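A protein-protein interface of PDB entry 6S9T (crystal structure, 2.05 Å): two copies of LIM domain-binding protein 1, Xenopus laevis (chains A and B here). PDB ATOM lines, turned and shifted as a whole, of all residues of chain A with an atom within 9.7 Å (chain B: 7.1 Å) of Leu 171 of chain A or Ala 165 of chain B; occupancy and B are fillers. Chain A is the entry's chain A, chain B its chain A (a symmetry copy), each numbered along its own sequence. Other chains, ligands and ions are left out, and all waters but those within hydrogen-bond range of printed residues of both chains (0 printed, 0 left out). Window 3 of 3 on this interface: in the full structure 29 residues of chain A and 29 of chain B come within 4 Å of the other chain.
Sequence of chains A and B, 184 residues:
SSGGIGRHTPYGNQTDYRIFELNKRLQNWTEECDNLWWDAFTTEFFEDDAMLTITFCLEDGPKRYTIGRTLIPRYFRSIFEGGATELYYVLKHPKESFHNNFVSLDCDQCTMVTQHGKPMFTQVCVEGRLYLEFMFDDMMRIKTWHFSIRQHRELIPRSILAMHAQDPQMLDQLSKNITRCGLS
The guanidinium group (NH1) of Arg 158 of chain A sits at hydrogen-bond distance from the backbone carbonyl oxygen (O) of Leu 174 of chain B, at 2.8 Å.
Of the printed residues of chain B, Leu 171 of chain A touches Ala 165 and Leu 171.
Of the printed residues of chain A, Ala 165 of chain B touches Leu 171 (3.6 Å) and Ser 175 (3.3 Å).
Printed residues of chain B within 4 Å of Ala 165 of chain A: Leu 171.
Printed residues of chain B within 4 Å of Ser 175 of chain A: Leu 161 (3.2 Å), Ala 162 (3.7 Å) and Ala 165 (3.3 Å).
His 164 of chain B touches none of the printed residues of chain A.
The nearest residue of chain A that does not touch Ala 165 of chain B is Asp 172 of chain A (5.6 Å).
The nearest printed residue of chain A that does not touch Leu 171 of chain B is Leu 161 of chain A (4.02 Å).
The backbone carbonyl oxygen of Leu 171 of chain A lies within hydrogen-bond range of the side-chain hydroxyl of Ser 175 of chain A (2.6 Å).
Leu 161 of chain A touches its own counterpart, Leu 161 of chain B.
Leu 161 of chain A touches Leu 174 of chain B, and with the chains exchanged Leu 174 of chain A touches Leu 161 of chain B.
Ala 165 of chain A touches Leu 171 of chain B, and with the chains exchanged Leu 171 of chain A touches Ala 165 of chain B.
Leu 171 of chain A touches its own counterpart, Leu 171 of chain B.
Positions printed for both chains: 160, 161, 162, 163, 164, 165, 166, 167, 168, 170, 171 and 174.
Of the 10 pairs that touch across the chains among the printed residues, 6 have their exchanged pair printed and touching as well.
Among the printed residues, merely in contact across the chains: Ser 175 of chain A with Leu 161 of chain B, Ser 175 of chain A with Ala 165 of chain B, Leu 161 of chain A with Leu 161 of chain B, Leu 171 of chain A with Ala 165 of chain B, Ala 165 of chain A with Leu 171 of chain B, Leu 171 of chain A with Leu 171 of chain B, Ser 175 of chain A with Ala 162 of chain B, Leu 161 of chain A with Leu 174 of chain B and Leu 174 of chain A with Leu 161 of chain B.
Printed residues of chain B that touch a printed residue of chain A: Leu 161, Ala 162, Ala 165, Leu 171 and Leu 174.
Hydrophobic or aromatic side chains of chain B within 4 Å of the printed part of chain A: Leu 161, Ala 162, Ala 165, Leu 171 and Leu 174.
Of the 21 printed residues of chain A, 6 touch a printed residue of chain B.
Among the printed residues, no Asp or Glu carboxylate lies within 4 Å of a Lys or Arg side-chain nitrogen of the other chain.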
ATOM      1  N   MET A 120       6.231   7.820  -2.906  1.00  0.00           N
ATOM      2  CA  MET A 120       6.168   6.489  -2.328  1.00  0.00           C
ATOM      3  C   MET A 120       7.287   5.595  -2.861  1.00  0.00           C
ATOM      4  O   MET A 120       7.503   4.511  -2.300  1.00  0.00           O
ATOM      5  CB  MET A 120       4.821   5.819  -2.602  1.00  0.00           C
ATOM      6  CG  MET A 120       3.611   6.592  -2.128  1.00  0.00           C
ATOM      7  SD  MET A 120       3.838   7.237  -0.294  1.00  0.00           S
ATOM      8  CE  MET A 120       2.207   8.302   0.066  1.00  0.00           C
ATOM      9  N   ILE A 156       7.193  -1.166  -1.062  1.00  0.00           N
ATOM     10  CA  ILE A 156       7.354   0.133  -0.360  1.00  0.00           C
ATOM     11  C   ILE A 156       8.737   0.166   0.255  1.00  0.00           C
ATOM     12  O   ILE A 156       9.090  -0.754   0.963  1.00  0.00           O
ATOM     13  CB  ILE A 156       6.268   0.237   0.745  1.00  0.00           C
ATOM     14  CG1 ILE A 156       4.917  -0.168   0.169  1.00  0.00           C
ATOM     15  CG2 ILE A 156       6.190   1.616   1.364  1.00  0.00           C
ATOM     16  CD1 ILE A 156       4.566   0.646  -1.034  1.00  0.00           C
ATOM     17  N   ARG A 158      11.287   0.819   3.151  1.00  0.00           N
ATOM     18  CA  ARG A 158      11.134   0.849   4.618  1.00  0.00           C
ATOM     19  C   ARG A 158      11.079   2.298   5.094  1.00  0.00           C
ATOM     20  O   ARG A 158      10.234   2.577   5.934  1.00  0.00           O
ATOM     21  CB  ARG A 158      12.259   0.093   5.303  1.00  0.00           C
ATOM     22  CG  ARG A 158      11.962  -0.144   6.772  1.00  0.00           C
ATOM     23  CD  ARG A 158      13.142  -0.750   7.479  1.00  0.00           C
ATOM     24  NE  ARG A 158      13.713  -1.915   6.806  1.00  0.00           N
ATOM     25  CZ  ARG A 158      13.163  -3.136   6.747  1.00  0.00           C
ATOM     26  NH1 ARG A 158      11.971  -3.382   7.259  1.00  0.00           N
ATOM     27  NH2 ARG A 158      13.802  -4.108   6.144  1.00  0.00           N
ATOM     28  N   ILE A 160       9.784   4.855   3.878  1.00  0.00           N
ATOM     29  CA  ILE A 160       8.433   5.443   3.703  1.00  0.00           C
ATOM     30  C   ILE A 160       7.492   4.861   4.758  1.00  0.00           C
ATOM     31  O   ILE A 160       6.671   5.628   5.300  1.00  0.00           O
ATOM     32  CB  ILE A 160       7.897   5.225   2.286  1.00  0.00           C
ATOM     33  CG1 ILE A 160       8.872   5.726   1.219  1.00  0.00           C
ATOM     34  CG2 ILE A 160       6.532   5.873   2.157  1.00  0.00           C
ATOM     35  CD1 ILE A 160       9.074   7.215   1.199  1.00  0.00           C
ATOM     36  N   LEU A 161       7.581   3.551   5.019  1.00  0.00           N
ATOM     37  CA  LEU A 161       6.869   2.922   6.152  1.00  0.00           C
ATOM     38  C   LEU A 161       7.239   3.702   7.422  1.00  0.00           C
ATOM     39  O   LEU A 161       6.316   4.181   8.113  1.00  0.00           O
ATOM     40  CB  LEU A 161       7.252   1.441   6.263  1.00  0.00           C
ATOM     41  CG  LEU A 161       6.428   0.651   7.280  1.00  0.00           C
ATOM     42  CD1 LEU A 161       6.183  -0.779   6.835  1.00  0.00           C
ATOM     43  CD2 LEU A 161       7.106   0.618   8.625  1.00  0.00           C
ATOM     44  N   ALA A 162       8.540   3.856   7.697  1.00  0.00           N
ATOM     45  CA  ALA A 162       9.063   4.469   8.946  1.00  0.00           C
ATOM     46  C   ALA A 162       8.447   5.860   9.130  1.00  0.00           C
ATOM     47  O   ALA A 162       7.964   6.176  10.206  1.00  0.00           O
ATOM     48  CB  ALA A 162      10.571   4.531   8.939  1.00  0.00           C
ATOM     49  N   MET A 163       8.396   6.681   8.075  1.00  0.00           N
ATOM     50  CA  MET A 163       7.995   8.062   8.297  1.00  0.00           C
ATOM     51  C   MET A 163       6.507   8.145   8.644  1.00  0.00           C
ATOM     52  O   MET A 163       6.066   9.121   9.245  1.00  0.00           O
ATOM     53  CB  MET A 163       8.365   8.935   7.097  1.00  0.00           C
ATOM     54  CG  MET A 163       7.466   8.775   5.903  1.00  0.00           C
ATOM     55  SD  MET A 163       8.165   9.953   4.483  1.00  0.00           S
ATOM     56  CE  MET A 163      10.106   9.544   4.348  1.00  0.00           C
ATOM     57  N   HIS A 164       5.718   7.128   8.282  1.00  0.00           N
ATOM     58  CA  HIS A 164       4.292   7.167   8.557  1.00  0.00           C
ATOM     59  C   HIS A 164       3.861   6.177   9.662  1.00  0.00           C
ATOM     60  O   HIS A 164       2.639   6.013   9.835  1.00  0.00           O
ATOM     61  CB  HIS A 164       3.585   6.881   7.238  1.00  0.00           C
ATOM     62  CG  HIS A 164       3.867   7.895   6.179  1.00  0.00           C
ATOM     63  ND1 HIS A 164       4.554   7.589   5.006  1.00  0.00           N
ATOM     64  CD2 HIS A 164       3.553   9.211   6.103  1.00  0.00           C
ATOM     65  CE1 HIS A 164       4.583   8.670   4.241  1.00  0.00           C
ATOM     66  NE2 HIS A 164       4.012   9.663   4.903  1.00  0.00           N
ATOM     67  N   ALA A 165       4.805   5.536  10.363  1.00  0.00           N
ATOM     68  CA  ALA A 165       4.576   4.395  11.295  1.00  0.00           C
ATOM     69  C   ALA A 165       3.584   4.767  12.412  1.00  0.00           C
ATOM     70  O   ALA A 165       2.842   3.874  12.866  1.00  0.00           O
ATOM     71  CB  ALA A 165       5.887   3.906  11.885  1.00  0.00           C
ATOM     72  N   GLN A 166       3.568   6.034  12.828  1.00  0.00           N
ATOM     73  CA  GLN A 166       2.726   6.522  13.954  1.00  0.00           C
ATOM     74  C   GLN A 166       1.510   7.294  13.393  1.00  0.00           C
ATOM     75  O   GLN A 166       0.901   8.059  14.149  1.00  0.00           O
ATOM     76  CB  GLN A 166       3.625   7.334  14.891  1.00  0.00           C
ATOM     77  CG  GLN A 166       4.980   6.676  15.132  1.00  0.00           C
ATOM     78  CD  GLN A 166       5.601   7.070  16.445  1.00  0.00           C
ATOM     79  OE1 GLN A 166       5.407   8.183  16.922  1.00  0.00           O
ATOM     80  NE2 GLN A 166       6.347   6.147  17.052  1.00  0.00           N
ATOM     81  N   ASP A 167       1.124   7.034  12.139  1.00  0.00           N
ATOM     82  CA  ASP A 167       0.127   7.813  11.351  1.00  0.00           C
ATOM     83  C   ASP A 167      -0.916   6.880  10.733  1.00  0.00           C
ATOM     84  O   ASP A 167      -0.783   6.415   9.598  1.00  0.00           O
ATOM     85  CB  ASP A 167       0.817   8.635  10.267  1.00  0.00           C
ATOM     86  CG  ASP A 167      -0.022   9.786   9.755  1.00  0.00           C
ATOM     87  OD1 ASP A 167      -1.277   9.727   9.826  1.00  0.00           O
ATOM     88  OD2 ASP A 167       0.591  10.724   9.295  1.00  0.00           O
ATOM     89  N   PRO A 168      -1.993   6.556  11.477  1.00  0.00           N
ATOM     90  CA  PRO A 168      -3.068   5.713  10.954  1.00  0.00           C
ATOM     91  C   PRO A 168      -3.600   6.161   9.591  1.00  0.00           C
ATOM     92  O   PRO A 168      -3.926   5.300   8.817  1.00  0.00           O
ATOM     93  CB  PRO A 168      -4.169   5.859  12.018  1.00  0.00           C
ATOM     94  CG  PRO A 168      -3.387   6.066  13.301  1.00  0.00           C
ATOM     95  CD  PRO A 168      -2.199   6.916  12.889  1.00  0.00           C
ATOM     96  N   GLN A 169      -3.712   7.472   9.355  1.00  0.00           N
ATOM     97  CA  GLN A 169      -4.276   7.995   8.090  1.00  0.00           C
ATOM     98  C   GLN A 169      -3.402   7.466   6.954  1.00  0.00           C
ATOM     99  O   GLN A 169      -3.880   6.804   6.047  1.00  0.00           O
ATOM    100  CB  GLN A 169      -4.372   9.523   8.127  1.00  0.00           C
ATOM    101  CG  GLN A 169      -4.756  10.162   6.799  1.00  0.00           C
ATOM    102  CD  GLN A 169      -5.221  11.588   6.966  1.00  0.00           C
ATOM    103  OE1 GLN A 169      -4.636  12.373   7.715  1.00  0.00           O
ATOM    104  NE2 GLN A 169      -6.308  11.924   6.289  1.00  0.00           N
ATOM    105  N   MET A 170      -2.102   7.724   7.044  1.00  0.00           N
ATOM    106  CA  MET A 170      -1.199   7.344   5.974  1.00  0.00           C
ATOM    107  C   MET A 170      -1.035   5.823   5.902  1.00  0.00           C
ATOM    108  O   MET A 170      -0.891   5.265   4.819  1.00  0.00           O
ATOM    109  CB  MET A 170       0.119   8.086   6.192  1.00  0.00           C
ATOM    110  CG  MET A 170      -0.029   9.582   6.067  1.00  0.00           C
ATOM    111  SD  MET A 170      -0.760   9.913   4.267  1.00  0.00           S
ATOM    112  CE  MET A 170       0.437   9.013   2.992  1.00  0.00           C
ATOM    113  N   LEU A 171      -1.086   5.134   7.049  1.00  0.00           N
ATOM    114  CA  LEU A 171      -0.983   3.684   7.038  1.00  0.00           C
ATOM    115  C   LEU A 171      -2.177   3.080   6.296  1.00  0.00           C
ATOM    116  O   LEU A 171      -1.961   2.116   5.557  1.00  0.00           O
ATOM    117  CB  LEU A 171      -0.876   3.138   8.467  1.00  0.00           C
ATOM    118  CG  LEU A 171       0.466   3.407   9.136  1.00  0.00           C
ATOM    119  CD1 LEU A 171       0.405   3.104  10.630  1.00  0.00           C
ATOM    120  CD2 LEU A 171       1.588   2.617   8.459  1.00  0.00           C
ATOM    121  N   ASP A 172      -3.371   3.654   6.456  1.00  0.00           N
ATOM    122  CA  ASP A 172      -4.558   3.308   5.622  1.00  0.00           C
ATOM    123  C   ASP A 172      -4.241   3.554   4.136  1.00  0.00           C
ATOM    124  O   ASP A 172      -4.480   2.643   3.298  1.00  0.00           O
ATOM    125  CB  ASP A 172      -5.801   4.118   6.014  1.00  0.00           C
ATOM    126  CG  ASP A 172      -6.363   3.691   7.359  1.00  0.00           C
ATOM    127  OD1 ASP A 172      -5.961   2.591   7.830  1.00  0.00           O
ATOM    128  OD2 ASP A 172      -7.212   4.448   7.915  1.00  0.00           O
ATOM    129  N   GLN A 173      -3.738   4.740   3.799  1.00  0.00           N
ATOM    130  CA  GLN A 173      -3.349   5.052   2.402  1.00  0.00           C
ATOM    131  C   GLN A 173      -2.419   3.940   1.878  1.00  0.00           C
ATOM    132  O   GLN A 173      -2.754   3.349   0.821  1.00  0.00           O
ATOM    133  CB  GLN A 173      -2.680   6.425   2.323  1.00  0.00           C
ATOM    134  CG  GLN A 173      -3.641   7.606   2.461  1.00  0.00           C
ATOM    135  CD  GLN A 173      -4.411   7.915   1.196  1.00  0.00           C
ATOM    136  OE1 GLN A 173      -5.570   7.551   1.085  1.00  0.00           O
ATOM    137  NE2 GLN A 173      -3.774   8.563   0.227  1.00  0.00           N
ATOM    138  N   LEU A 174      -1.323   3.660   2.610  1.00  0.00           N
ATOM    139  CA  LEU A 174      -0.211   2.756   2.188  1.00  0.00           C
ATOM    140  C   LEU A 174      -0.660   1.294   2.163  1.00  0.00           C
ATOM    141  O   LEU A 174      -0.026   0.504   1.418  1.00  0.00           O
ATOM    142  CB  LEU A 174       0.974   2.880   3.142  1.00  0.00           C
ATOM    143  CG  LEU A 174       1.862   4.105   2.973  1.00  0.00           C
ATOM    144  CD1 LEU A 174       2.806   4.225   4.155  1.00  0.00           C
ATOM    145  CD2 LEU A 174       2.670   4.045   1.691  1.00  0.00           C
ATOM    146  N   SER A 175      -1.685   0.952   2.944  1.00  0.00           N
ATOM    147  CA  SER A 175      -2.164  -0.441   3.136  1.00  0.00           C
ATOM    148  C   SER A 175      -2.962  -0.894   1.909  1.00  0.00           C
ATOM    149  O   SER A 175      -3.048  -2.098   1.696  1.00  0.00           O
ATOM    150  CB  SER A 175      -2.953  -0.603   4.426  1.00  0.00           C
ATOM    151  OG  SER A 175      -2.076  -0.516   5.547  1.00  0.00           O
ATOM    152  N   LYS A 176      -3.424   0.043   1.086  1.00  0.00           N
ATOM    153  CA  LYS A 176      -4.249  -0.251  -0.121  1.00  0.00           C
ATOM    154  C   LYS A 176      -3.380  -0.392  -1.383  1.00  0.00           C
ATOM    155  O   LYS A 176      -2.503   0.462  -1.611  1.00  0.00           O
ATOM    156  CB  LYS A 176      -5.300   0.849  -0.261  1.00  0.00           C
ATOM    157  CG  LYS A 176      -6.234   0.950   0.935  1.00  0.00           C
ATOM    158  CD  LYS A 176      -7.315   2.003   0.799  1.00  0.00           C
ATOM    159  CE  LYS A 176      -8.541   1.620   1.595  1.00  0.00           C
ATOM    160  NZ  LYS A 176      -9.068   2.778   2.345  1.00  0.00           N
ATOM    161  N   ASN A 177      -3.649  -1.416  -2.201  1.00  0.00           N
ATOM    162  CA  ASN A 177      -2.964  -1.627  -3.501  1.00  0.00           C
ATOM    163  C   ASN A 177      -3.377  -0.549  -4.510  1.00  0.00           C
ATOM    164  O   ASN A 177      -4.456  -0.046  -4.394  1.00  0.00           O
ATOM    165  CB  ASN A 177      -3.274  -2.968  -4.158  1.00  0.00           C
ATOM    166  CG  ASN A 177      -2.444  -4.112  -3.633  1.00  0.00           C
ATOM    167  OD1 ASN A 177      -1.380  -3.914  -3.043  1.00  0.00           O
ATOM    168  ND2 ASN A 177      -2.936  -5.317  -3.858  1.00  0.00           N
ATOM    169  N   ILE B 160       2.480  -7.020   3.545  1.00  0.00           N
ATOM    170  CA  ILE B 160       3.092  -7.186   4.885  1.00  0.00           C
ATOM    171  C   ILE B 160       2.843  -5.925   5.711  1.00  0.00           C
ATOM    172  O   ILE B 160       2.555  -6.060   6.918  1.00  0.00           O
ATOM    173  CB  ILE B 160       4.585  -7.515   4.792  1.00  0.00           C
ATOM    174  CG1 ILE B 160       4.853  -8.726   3.896  1.00  0.00           C
ATOM    175  CG2 ILE B 160       5.147  -7.705   6.188  1.00  0.00           C
ATOM    176  CD1 ILE B 160       4.328 -10.030   4.425  1.00  0.00           C
ATOM    177  N   LEU B 161       2.975  -4.742   5.101  1.00  0.00           N
ATOM    178  CA  LEU B 161       2.566  -3.473   5.738  1.00  0.00           C
ATOM    179  C   LEU B 161       1.106  -3.631   6.189  1.00  0.00           C
ATOM    180  O   LEU B 161       0.832  -3.427   7.390  1.00  0.00           O
ATOM    181  CB  LEU B 161       2.734  -2.306   4.757  1.00  0.00           C
ATOM    182  CG  LEU B 161       2.522  -0.925   5.376  1.00  0.00           C
ATOM    183  CD1 LEU B 161       3.434   0.124   4.768  1.00  0.00           C
ATOM    184  CD2 LEU B 161       1.097  -0.466   5.211  1.00  0.00           C
ATOM    185  N   ALA B 162       0.213  -4.018   5.270  1.00  0.00           N
ATOM    186  CA  ALA B 162      -1.252  -4.094   5.508  1.00  0.00           C
ATOM    187  C   ALA B 162      -1.526  -4.976   6.731  1.00  0.00           C
ATOM    188  O   ALA B 162      -2.281  -4.585   7.608  1.00  0.00           O
ATOM    189  CB  ALA B 162      -1.982  -4.598   4.289  1.00  0.00           C
ATOM    190  N   MET B 163      -0.875  -6.140   6.837  1.00  0.00           N
ATOM    191  CA  MET B 163      -1.280  -7.061   7.888  1.00  0.00           C
ATOM    192  C   MET B 163      -0.883  -6.521   9.264  1.00  0.00           C
ATOM    193  O   MET B 163      -1.462  -6.915  10.274  1.00  0.00           O
ATOM    194  CB  MET B 163      -0.725  -8.461   7.627  1.00  0.00           C
ATOM    195  CG  MET B 163       0.739  -8.623   7.931  1.00  0.00           C
ATOM    196  SD  MET B 163       1.227 -10.480   7.474  1.00  0.00           S
ATOM    197  CE  MET B 163       0.536 -10.784   5.634  1.00  0.00           C
ATOM    198  N   HIS B 164       0.096  -5.612   9.326  1.00  0.00           N
ATOM    199  CA  HIS B 164       0.537  -5.089  10.608  1.00  0.00           C
ATOM    200  C   HIS B 164       0.123  -3.617  10.835  1.00  0.00           C
ATOM    201  O   HIS B 164       0.612  -3.035  11.821  1.00  0.00           O
ATOM    202  CB  HIS B 164       2.050  -5.263  10.654  1.00  0.00           C
ATOM    203  CG  HIS B 164       2.487  -6.687  10.575  1.00  0.00           C
ATOM    204  ND1 HIS B 164       3.222  -7.193   9.504  1.00  0.00           N
ATOM    205  CD2 HIS B 164       2.307  -7.722  11.433  1.00  0.00           C
ATOM    206  CE1 HIS B 164       3.518  -8.460   9.756  1.00  0.00           C
ATOM    207  NE2 HIS B 164       2.945  -8.800  10.901  1.00  0.00           N
ATOM    208  N   ALA B 165      -0.715  -3.037   9.967  1.00  0.00           N
ATOM    209  CA  ALA B 165      -1.035  -1.582   9.903  1.00  0.00           C
ATOM    210  C   ALA B 165      -1.596  -1.068  11.240  1.00  0.00           C
ATOM    211  O   ALA B 165      -1.352   0.109  11.570  1.00  0.00           O
ATOM    212  CB  ALA B 165      -2.001  -1.291   8.768  1.00  0.00           C
ATOM    213  N   GLN B 166      -2.312  -1.917  11.978  1.00  0.00           N
ATOM    214  CA  GLN B 166      -2.988  -1.539  13.249  1.00  0.00           C
ATOM    215  C   GLN B 166      -2.175  -2.081  14.447  1.00  0.00           C
ATOM    216  O   GLN B 166      -2.739  -2.176  15.543  1.00  0.00           O
ATOM    217  CB  GLN B 166      -4.434  -2.039  13.175  1.00  0.00           C
ATOM    218  CG  GLN B 166      -5.082  -1.784  11.818  1.00  0.00           C
ATOM    219  CD  GLN B 166      -6.581  -1.677  11.891  1.00  0.00           C
ATOM    220  OE1 GLN B 166      -7.215  -2.317  12.724  1.00  0.00           O
ATOM    221  NE2 GLN B 166      -7.163  -0.848  11.026  1.00  0.00           N
ATOM    222  N   ASP B 167      -0.876  -2.342  14.261  1.00  0.00           N
ATOM    223  CA  ASP B 167       0.017  -3.061  15.211  1.00  0.00           C
ATOM    224  C   ASP B 167       1.304  -2.268  15.444  1.00  0.00           C
ATOM    225  O   ASP B 167       2.318  -2.457  14.768  1.00  0.00           O
ATOM    226  CB  ASP B 167       0.339  -4.461  14.698  1.00  0.00           C
ATOM    227  CG  ASP B 167       0.819  -5.407  15.778  1.00  0.00           C
ATOM    228  OD1 ASP B 167       1.375  -4.949  16.809  1.00  0.00           O
ATOM    229  OD2 ASP B 167       0.626  -6.585  15.573  1.00  0.00           O
ATOM    230  N   PRO B 168       1.298  -1.326  16.409  1.00  0.00           N
ATOM    231  CA  PRO B 168       2.495  -0.552  16.741  1.00  0.00           C
ATOM    232  C   PRO B 168       3.742  -1.408  16.975  1.00  0.00           C
ATOM    233  O   PRO B 168       4.794  -0.962  16.603  1.00  0.00           O
ATOM    234  CB  PRO B 168       2.096   0.158  18.045  1.00  0.00           C
ATOM    235  CG  PRO B 168       0.600   0.359  17.889  1.00  0.00           C
ATOM    236  CD  PRO B 168       0.122  -0.897  17.182  1.00  0.00           C
ATOM    237  N   MET B 170       4.667  -4.354  15.695  1.00  0.00           N
ATOM    238  CA  MET B 170       5.234  -4.813  14.442  1.00  0.00           C
ATOM    239  C   MET B 170       5.671  -3.635  13.567  1.00  0.00           C
ATOM    240  O   MET B 170       6.664  -3.727  12.853  1.00  0.00           O
ATOM    241  CB  MET B 170       4.205  -5.720  13.770  1.00  0.00           C
ATOM    242  CG  MET B 170       3.933  -6.976  14.559  1.00  0.00           C
ATOM    243  SD  MET B 170       5.670  -7.881  14.769  1.00  0.00           S
ATOM    244  CE  MET B 170       6.423  -8.094  12.964  1.00  0.00           C
ATOM    245  N   LEU B 171       4.953  -2.507  13.635  1.00  0.00           N
ATOM    246  CA  LEU B 171       5.346  -1.340  12.862  1.00  0.00           C
ATOM    247  C   LEU B 171       6.709  -0.832  13.336  1.00  0.00           C
ATOM    248  O   LEU B 171       7.505  -0.447  12.477  1.00  0.00           O
ATOM    249  CB  LEU B 171       4.276  -0.245  12.953  1.00  0.00           C
ATOM    250  CG  LEU B 171       3.004  -0.553  12.174  1.00  0.00           C
ATOM    251  CD1 LEU B 171       1.888   0.421  12.538  1.00  0.00           C
ATOM    252  CD2 LEU B 171       3.265  -0.553  10.666  1.00  0.00           C
ATOM    253  N   LEU B 174       9.177  -3.308  11.778  1.00  0.00           N
ATOM    254  CA  LEU B 174       9.266  -3.090  10.301  1.00  0.00           C
ATOM    255  C   LEU B 174       9.937  -1.755   9.976  1.00  0.00           C
ATOM    256  O   LEU B 174      10.488  -1.641   8.851  1.00  0.00           O
ATOM    257  CB  LEU B 174       7.876  -3.096   9.673  1.00  0.00           C
ATOM    258  CG  LEU B 174       7.226  -4.458   9.465  1.00  0.00           C
ATOM    259  CD1 LEU B 174       5.764  -4.283   9.102  1.00  0.00           C
ATOM    260  CD2 LEU B 174       7.920  -5.254   8.376  1.00  0.00           C
